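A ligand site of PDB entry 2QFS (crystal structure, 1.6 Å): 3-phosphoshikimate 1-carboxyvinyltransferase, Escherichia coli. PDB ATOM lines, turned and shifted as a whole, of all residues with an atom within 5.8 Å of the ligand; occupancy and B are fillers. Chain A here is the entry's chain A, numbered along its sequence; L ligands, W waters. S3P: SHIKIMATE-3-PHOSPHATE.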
ATOM      1  N   LYS A  22       6.813  15.505  -2.873  1.00  0.00           N
ATOM      2  CA  LYS A  22       5.607  14.751  -3.209  1.00  0.00           C
ATOM      3  C   LYS A  22       4.929  15.323  -4.449  1.00  0.00           C
ATOM      4  O   LYS A  22       4.499  14.572  -5.318  1.00  0.00           O
ATOM      5  CB  LYS A  22       4.627  14.784  -2.017  1.00  0.00           C
ATOM      6  CG  LYS A  22       3.263  14.089  -2.295  1.00  0.00           C
ATOM      7  CD  LYS A  22       2.115  15.104  -2.389  1.00  0.00           C
ATOM      8  CE  LYS A  22       1.742  15.600  -0.992  1.00  0.00           C
ATOM      9  NZ  LYS A  22       0.873  16.791  -1.012  1.00  0.00           N
ATOM     10  N   SER A  23       4.865  16.647  -4.529  1.00  0.00           N
ATOM     11  CA  SER A  23       4.213  17.316  -5.667  1.00  0.00           C
ATOM     12  C   SER A  23       4.889  16.989  -6.990  1.00  0.00           C
ATOM     13  O   SER A  23       4.242  16.667  -7.973  1.00  0.00           O
ATOM     14  CB  SER A  23       4.198  18.841  -5.444  1.00  0.00           C
ATOM     15  OG  SER A  23       3.374  19.189  -4.325  1.00  0.00           O
ATOM     16  N   ARG A  27       3.496  14.107 -10.171  1.00  0.00           N
ATOM     17  CA  ARG A  27       3.331  14.642 -11.509  1.00  0.00           C
ATOM     18  C   ARG A  27       4.303  13.921 -12.454  1.00  0.00           C
ATOM     19  O   ARG A  27       3.932  13.500 -13.562  1.00  0.00           O
ATOM     20  CB  ARG A  27       3.661  16.136 -11.545  1.00  0.00           C
ATOM     21  CG  ARG A  27       2.596  17.039 -10.950  1.00  0.00           C
ATOM     22  CD  ARG A  27       3.193  18.428 -10.745  1.00  0.00           C
ATOM     23  NE  ARG A  27       2.258  19.462 -10.335  1.00  0.00           N
ATOM     24  CZ  ARG A  27       1.736  19.583  -9.123  1.00  0.00           C
ATOM     25  NH1 ARG A  27       0.902  20.589  -8.863  1.00  0.00           N
ATOM     26  NH2 ARG A  27       2.032  18.701  -8.161  1.00  0.00           N
ATOM     27  N   THR A  97      -3.031  14.673  -4.956  1.00  0.00           N
ATOM     28  CA  THR A  97      -2.254  14.770  -6.177  1.00  0.00           C
ATOM     29  C   THR A  97      -2.501  13.589  -7.110  1.00  0.00           C
ATOM     30  O   THR A  97      -2.396  13.746  -8.326  1.00  0.00           O
ATOM     31  CB  THR A  97      -0.738  14.913  -5.881  1.00  0.00           C
ATOM     32  OG1 THR A  97      -0.263  13.787  -5.128  1.00  0.00           O
ATOM     33  CG2 THR A  97      -0.480  16.193  -5.086  1.00  0.00           C
ATOM     34  N   ARG A 100      -6.954  13.774  -7.953  1.00  0.00           N
ATOM     35  CA  ARG A 100      -7.347  14.788  -8.914  1.00  0.00           C
ATOM     36  C   ARG A 100      -6.671  14.562 -10.265  1.00  0.00           C
ATOM     37  O   ARG A 100      -7.373  14.544 -11.287  1.00  0.00           O
ATOM     38  CB  ARG A 100      -7.042  16.203  -8.373  1.00  0.00           C
ATOM     39  CG  ARG A 100      -8.068  16.769  -7.376  1.00  0.00           C
ATOM     40  CD  ARG A 100      -8.095  16.028  -6.029  1.00  0.00           C
ATOM     41  NE  ARG A 100      -9.058  16.590  -5.081  1.00  0.00           N
ATOM     42  CZ  ARG A 100      -8.773  17.546  -4.211  1.00  0.00           C
ATOM     43  NH1 ARG A 100      -9.705  18.019  -3.372  1.00  0.00           N
ATOM     44  NH2 ARG A 100      -7.545  18.029  -4.143  1.00  0.00           N
ATOM     45  N   VAL A 168     -11.092  26.917  -4.980  1.00  0.00           N
ATOM     46  CA  VAL A 168     -10.966  25.958  -3.868  1.00  0.00           C
ATOM     47  C   VAL A 168      -9.677  25.140  -3.927  1.00  0.00           C
ATOM     48  O   VAL A 168      -9.031  24.906  -2.901  1.00  0.00           O
ATOM     49  CB  VAL A 168     -12.212  25.045  -3.807  1.00  0.00           C
ATOM     50  CG1 VAL A 168     -12.029  23.939  -2.770  1.00  0.00           C
ATOM     51  CG2 VAL A 168     -13.424  25.884  -3.444  1.00  0.00           C
ATOM     52  N   SER A 169      -9.327  24.664  -5.113  1.00  0.00           N
ATOM     53  CA  SER A 169      -8.075  23.916  -5.264  1.00  0.00           C
ATOM     54  C   SER A 169      -7.420  24.141  -6.610  1.00  0.00           C
ATOM     55  O   SER A 169      -8.085  24.161  -7.659  1.00  0.00           O
ATOM     56  CB  SER A 169      -8.320  22.403  -5.063  1.00  0.00           C
ATOM     57  OG  SER A 169      -7.093  21.688  -5.188  1.00  0.00           O
ATOM     58  N   SER A 170      -6.110  24.321  -6.571  1.00  0.00           N
ATOM     59  CA  SER A 170      -5.357  24.464  -7.805  1.00  0.00           C
ATOM     60  C   SER A 170      -5.206  23.064  -8.435  1.00  0.00           C
ATOM     61  O   SER A 170      -4.909  22.960  -9.622  1.00  0.00           O
ATOM     62  CB  SER A 170      -3.957  25.037  -7.529  1.00  0.00           C
ATOM     63  OG  SER A 170      -3.125  24.096  -6.859  1.00  0.00           O
ATOM     64  N   GLN A 171      -5.435  22.004  -7.654  1.00  0.00           N
ATOM     65  CA  GLN A 171      -5.283  20.656  -8.191  1.00  0.00           C
ATOM     66  C   GLN A 171      -6.195  20.317  -9.342  1.00  0.00           C
ATOM     67  O   GLN A 171      -5.879  19.455 -10.167  1.00  0.00           O
ATOM     68  CB  GLN A 171      -5.438  19.622  -7.076  1.00  0.00           C
ATOM     69  CG  GLN A 171      -4.300  19.706  -6.044  1.00  0.00           C
ATOM     70  CD  GLN A 171      -4.275  18.524  -5.090  1.00  0.00           C
ATOM     71  OE1 GLN A 171      -5.078  17.616  -5.173  1.00  0.00           O
ATOM     72  NE2 GLN A 171      -3.300  18.538  -4.171  1.00  0.00           N
ATOM     73  N   THR A 174      -4.500  21.895 -12.370  1.00  0.00           N
ATOM     74  CA  THR A 174      -3.329  21.078 -12.657  1.00  0.00           C
ATOM     75  C   THR A 174      -3.716  19.807 -13.411  1.00  0.00           C
ATOM     76  O   THR A 174      -3.063  19.422 -14.393  1.00  0.00           O
ATOM     77  CB  THR A 174      -2.599  20.687 -11.337  1.00  0.00           C
ATOM     78  OG1 THR A 174      -1.739  21.775 -10.971  1.00  0.00           O
ATOM     79  CG2 THR A 174      -1.769  19.395 -11.508  1.00  0.00           C
ATOM     80  N   VAL A 196      -6.456  29.939  -6.382  1.00  0.00           N
ATOM     81  CA  VAL A 196      -5.684  29.773  -5.154  1.00  0.00           C
ATOM     82  C   VAL A 196      -4.511  28.838  -5.403  1.00  0.00           C
ATOM     83  O   VAL A 196      -4.451  28.149  -6.435  1.00  0.00           O
ATOM     84  CB  VAL A 196      -6.546  29.205  -3.999  1.00  0.00           C
ATOM     85  CG1 VAL A 196      -7.680  30.179  -3.649  1.00  0.00           C
ATOM     86  CG2 VAL A 196      -7.088  27.823  -4.357  1.00  0.00           C
ATOM     87  N   SER A 197      -3.558  28.850  -4.479  1.00  0.00           N
ATOM     88  CA  SER A 197      -2.354  28.030  -4.555  1.00  0.00           C
ATOM     89  C   SER A 197      -1.675  28.132  -5.921  1.00  0.00           C
ATOM     90  O   SER A 197      -1.207  27.152  -6.490  1.00  0.00           O
ATOM     91  CB  SER A 197      -2.724  26.575  -4.248  1.00  0.00           C
ATOM     92  OG  SER A 197      -3.181  26.502  -2.907  1.00  0.00           O
ATOM     93  N   TYR A 200       1.517  26.200  -7.390  1.00  0.00           N
ATOM     94  CA  TYR A 200       1.451  24.809  -7.805  1.00  0.00           C
ATOM     95  C   TYR A 200       1.156  24.659  -9.287  1.00  0.00           C
ATOM     96  O   TYR A 200       1.527  23.646  -9.901  1.00  0.00           O
ATOM     97  CB  TYR A 200       0.436  24.020  -6.974  1.00  0.00           C
ATOM     98  CG  TYR A 200       0.937  23.794  -5.570  1.00  0.00           C
ATOM     99  CD1 TYR A 200       0.585  24.664  -4.530  1.00  0.00           C
ATOM    100  CD2 TYR A 200       1.791  22.716  -5.279  1.00  0.00           C
ATOM    101  CE1 TYR A 200       1.072  24.472  -3.228  1.00  0.00           C
ATOM    102  CE2 TYR A 200       2.288  22.514  -3.977  1.00  0.00           C
ATOM    103  CZ  TYR A 200       1.907  23.397  -2.967  1.00  0.00           C
ATOM    104  OH  TYR A 200       2.327  23.211  -1.673  1.00  0.00           O
ATOM    105  N   ILE A 203       4.425  24.714 -10.923  1.00  0.00           N
ATOM    106  CA  ILE A 203       5.101  23.420 -10.833  1.00  0.00           C
ATOM    107  C   ILE A 203       4.610  22.513 -11.983  1.00  0.00           C
ATOM    108  O   ILE A 203       5.388  21.859 -12.656  1.00  0.00           O
ATOM    109  CB  ILE A 203       4.785  22.723  -9.473  1.00  0.00           C
ATOM    110  CG1 ILE A 203       5.389  23.524  -8.325  1.00  0.00           C
ATOM    111  CG2 ILE A 203       5.332  21.292  -9.462  1.00  0.00           C
ATOM    112  CD1 ILE A 203       5.122  22.895  -6.965  1.00  0.00           C
ATOM    113  N   THR A 204       3.294  22.478 -12.196  1.00  0.00           N
ATOM    114  CA  THR A 204       2.700  21.661 -13.252  1.00  0.00           C
ATOM    115  C   THR A 204       3.212  22.037 -14.632  1.00  0.00           C
ATOM    116  O   THR A 204       3.570  21.163 -15.409  1.00  0.00           O
ATOM    117  CB  THR A 204       1.169  21.783 -13.193  1.00  0.00           C
ATOM    118  OG1 THR A 204       0.751  21.319 -11.901  1.00  0.00           O
ATOM    119  CG2 THR A 204       0.486  20.952 -14.285  1.00  0.00           C
ATOM    120  N   PRO A 312       0.154  27.475   1.344  1.00  0.00           N
ATOM    121  CA  PRO A 312      -0.772  26.880   2.305  1.00  0.00           C
ATOM    122  C   PRO A 312      -0.285  25.746   3.186  1.00  0.00           C
ATOM    123  O   PRO A 312      -0.713  25.647   4.345  1.00  0.00           O
ATOM    124  CB  PRO A 312      -1.966  26.483   1.439  1.00  0.00           C
ATOM    125  CG  PRO A 312      -1.324  26.142   0.124  1.00  0.00           C
ATOM    126  CD  PRO A 312      -0.303  27.269  -0.038  1.00  0.00           C
ATOM    127  N   ASP A 313       0.576  24.887   2.637  1.00  0.00           N
ATOM    128  CA  ASP A 313       1.094  23.734   3.389  1.00  0.00           C
ATOM    129  C   ASP A 313       2.172  24.179   4.360  1.00  0.00           C
ATOM    130  O   ASP A 313       2.055  23.951   5.577  1.00  0.00           O
ATOM    131  CB  ASP A 313       1.642  22.653   2.444  1.00  0.00           C
ATOM    132  CG  ASP A 313       0.553  21.949   1.637  1.00  0.00           C
ATOM    133  OD1 ASP A 313       0.931  21.151   0.760  1.00  0.00           O
ATOM    134  OD2 ASP A 313      -0.652  22.176   1.856  1.00  0.00           O
ATOM    135  N   ASN A 336      -8.895  27.084   2.222  1.00  0.00           N
ATOM    136  CA  ASN A 336      -8.834  25.676   1.818  1.00  0.00           C
ATOM    137  C   ASN A 336      -8.118  24.701   2.739  1.00  0.00           C
ATOM    138  O   ASN A 336      -8.119  23.488   2.498  1.00  0.00           O
ATOM    139  CB  ASN A 336      -8.454  25.520   0.320  1.00  0.00           C
ATOM    140  CG  ASN A 336      -6.981  25.654   0.053  1.00  0.00           C
ATOM    141  OD1 ASN A 336      -6.131  25.765   0.961  1.00  0.00           O
ATOM    142  ND2 ASN A 336      -6.648  25.623  -1.245  1.00  0.00           N
ATOM    143  N   LYS A 340      -8.652  19.879   3.160  1.00  0.00           N
ATOM    144  CA  LYS A 340      -7.465  19.075   2.911  1.00  0.00           C
ATOM    145  C   LYS A 340      -7.406  17.769   3.734  1.00  0.00           C
ATOM    146  O   LYS A 340      -8.445  17.180   3.971  1.00  0.00           O
ATOM    147  CB  LYS A 340      -6.231  19.961   3.055  1.00  0.00           C
ATOM    148  CG  LYS A 340      -6.158  20.914   1.843  1.00  0.00           C
ATOM    149  CD  LYS A 340      -5.103  21.985   1.944  1.00  0.00           C
ATOM    150  CE  LYS A 340      -4.985  22.639   0.555  1.00  0.00           C
ATOM    151  NZ  LYS A 340      -4.042  23.760   0.534  1.00  0.00           N
ATOM    152  N   GLU A 341      -6.219  17.327   4.156  1.00  0.00           N
ATOM    153  CA  GLU A 341      -6.111  16.064   4.894  1.00  0.00           C
ATOM    154  C   GLU A 341      -7.106  15.978   6.063  1.00  0.00           C
ATOM    155  O   GLU A 341      -7.593  14.881   6.388  1.00  0.00           O
ATOM    156  CB  GLU A 341      -4.667  15.837   5.365  1.00  0.00           C
ATOM    157  CG  GLU A 341      -3.767  15.268   4.238  1.00  0.00           C
ATOM    158  CD  GLU A 341      -3.184  16.321   3.260  1.00  0.00           C
ATOM    159  OE1 GLU A 341      -3.779  17.418   3.039  1.00  0.00           O
ATOM    160  OE2 GLU A 341      -2.135  16.031   2.668  1.00  0.00           O
ATOM    161  N   ARG A 344      -7.917  21.716   8.569  1.00  0.00           N
ATOM    162  CA  ARG A 344      -6.736  22.193   9.269  1.00  0.00           C
ATOM    163  C   ARG A 344      -6.944  23.453  10.106  1.00  0.00           C
ATOM    164  O   ARG A 344      -6.204  23.671  11.056  1.00  0.00           O
ATOM    165  CB  ARG A 344      -5.587  22.366   8.266  1.00  0.00           C
ATOM    166  CG  ARG A 344      -5.073  21.010   7.778  1.00  0.00           C
ATOM    167  CD  ARG A 344      -4.190  21.103   6.533  1.00  0.00           C
ATOM    168  NE  ARG A 344      -3.373  19.901   6.426  1.00  0.00           N
ATOM    169  CZ  ARG A 344      -2.575  19.630   5.391  1.00  0.00           C
ATOM    170  NH1 ARG A 344      -1.840  18.518   5.391  1.00  0.00           N
ATOM    171  NH2 ARG A 344      -2.522  20.481   4.357  1.00  0.00           N
ATOM    172  N   ARG A 386       0.901  16.596   8.458  1.00  0.00           N
ATOM    173  CA  ARG A 386       1.387  17.910   8.880  1.00  0.00           C
ATOM    174  C   ARG A 386       1.034  18.316  10.296  1.00  0.00           C
ATOM    175  O   ARG A 386       1.740  19.109  10.895  1.00  0.00           O
ATOM    176  CB  ARG A 386       0.975  18.988   7.873  1.00  0.00           C
ATOM    177  CG  ARG A 386       1.595  18.739   6.481  1.00  0.00           C
ATOM    178  CD  ARG A 386       1.622  19.989   5.568  1.00  0.00           C
ATOM    179  NE  ARG A 386       1.985  19.518   4.220  1.00  0.00           N
ATOM    180  CZ  ARG A 386       3.183  19.069   3.855  1.00  0.00           C
ATOM    181  NH1 ARG A 386       3.328  18.616   2.614  1.00  0.00           N
ATOM    182  NH2 ARG A 386       4.242  19.134   4.669  1.00  0.00           N
HETATM  183  C1  S3P L   1      -0.568  20.418  -4.278  1.00  0.00           C
HETATM  184  C2  S3P L   1      -1.344  21.608  -4.270  1.00  0.00           C
HETATM  185  C3  S3P L   1      -1.929  22.144  -2.978  1.00  0.00           C
HETATM  186  C4  S3P L   1      -1.249  21.562  -1.734  1.00  0.00           C
HETATM  187  C5  S3P L   1      -1.172  20.040  -1.848  1.00  0.00           C
HETATM  188  C6  S3P L   1      -0.281  19.724  -3.059  1.00  0.00           C
HETATM  189  C7  S3P L   1      -0.029  19.898  -5.588  1.00  0.00           C
HETATM  190  O1  S3P L   1      -3.405  21.926  -2.944  1.00  0.00           O
HETATM  191  O2  S3P L   1      -1.986  21.992  -0.581  1.00  0.00           O
HETATM  192  O3  S3P L   1      -0.599  19.479  -0.677  1.00  0.00           O
HETATM  193  O4  S3P L   1      -0.688  20.129  -6.615  1.00  0.00           O
HETATM  194  O5  S3P L   1       1.004  19.270  -5.572  1.00  0.00           O
HETATM  195  P1  S3P L   1      -4.513  23.102  -3.201  1.00  0.00           P
HETATM  196  O6  S3P L   1      -4.379  23.576  -4.607  1.00  0.00           O
HETATM  197  O7  S3P L   1      -4.225  24.189  -2.220  1.00  0.00           O
HETATM  198  O8  S3P L   1      -5.841  22.451  -2.993  1.00  0.00           O
HETATM  199  O   HOH W   1      -2.077  21.973  -8.328  1.00  0.00           O
HETATM  200  O   HOH W   2      -6.005  19.805  -2.021  1.00  0.00           O
HETATM  201  O   HOH W   3      -1.644  17.866  -8.144  1.00  0.00           O
HETATM  202  O   HOH W   4      -8.087  22.420  -1.607  1.00  0.00           O
HETATM  203  O   HOH W   5      -3.384  19.250   0.835  1.00  0.00           O
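The side-chain hydroxyl (OG) of Ser 197 lies within hydrogen-bond range of an oxygen (O7) of the ligand (2.6 Å).
The backbone NH of Ser 170 lies within hydrogen-bond range of an oxygen (O6) of the ligand, at 2.7 Å.
The side-chain hydroxyl (OG) of Ser 170 is in hydrogen-bond range of an oxygen (O6) of the ligand (2.6 Å).
O8 of the ligand lies within hydrogen-bond range of OG of Ser 169 (2.6 Å).
OG of Ser 23 lies within hydrogen-bond range of O5 of the ligand (2.7 Å).
O3 of the ligand sits at hydrogen-bond distance from OD1 of Asp 313, 2.7 Å away.
An oxygen (O4) of the ligand lies within salt-bridge range of the guanidinium group of Arg 27 (2.8 Å).
The side-chain amino group (NZ) of Lys 340 is in salt-bridge range of an oxygen (O7) of the ligand.
ND2 of Asn 336 is in hydrogen-bond range of O7 of the ligand (3.0 Å).
NZ of Lys 22 lies within hydrogen-bond range of O3 of the ligand.
The side-chain hydroxyl of Ser 169 is in hydrogen-bond range of the backbone NH of Gln 171 (3.0 Å).
OD2 of Asp 313 is in salt-bridge range of NZ of Lys 340 (3.97 Å).
OD1 of Asp 313 lies within hydrogen-bond range of OH of Tyr 200, 3.5 Å away.
The guanidinium group of Arg 386 is in salt-bridge range of the side-chain carboxylate of Asp 313, 3.95 Å away.
The guanidinium group of Arg 27 sits at hydrogen-bond distance from the backbone carbonyl oxygen of Tyr 200, at 3.3 Å.
The side-chain amide nitrogen (ND2) of Asn 336 sits at hydrogen-bond distance from the backbone carbonyl oxygen (O) of Val 168.
NH2 of Arg 100 is in hydrogen-bond range of OE1 of Gln 171, at 2.7 Å.
O of Tyr 200 sits at hydrogen-bond distance from OG1 of Thr 204 (3.2 Å).
Residues that only touch the ligand: Thr 97, Gln 171 and Tyr 200.
Of the 22 residues printed, 12 come within 4 Å of the ligand.
The nearest printed residue that does not touch the ligand is Val 168 (4.03 Å).
Water W4 lies within hydrogen-bond range of O8 of the ligand (2.6 Å) and O of Val 168 (3.0 Å).
Water W2 lies within hydrogen-bond range of an oxygen (O8) of the ligand (2.8 Å) and the guanidinium group of Arg 100 (3.2 Å).
Water W1 lies within hydrogen-bond range of the side-chain hydroxyl (OG1) of Thr 174 (2.7 Å), the side-chain hydroxyl (OG) of Ser 170 (2.8 Å), an oxygen (O4) of the ligand (2.9 Å), the guanidinium group (NH1) of Arg 27 (3.3 Å) and the backbone NH (N) of Gln 171 (3.4 Å).
Water W5 bridges the side-chain carboxylate of Glu 341 (2.9 Å) and an oxygen (O3) of the ligand (3.2 Å).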
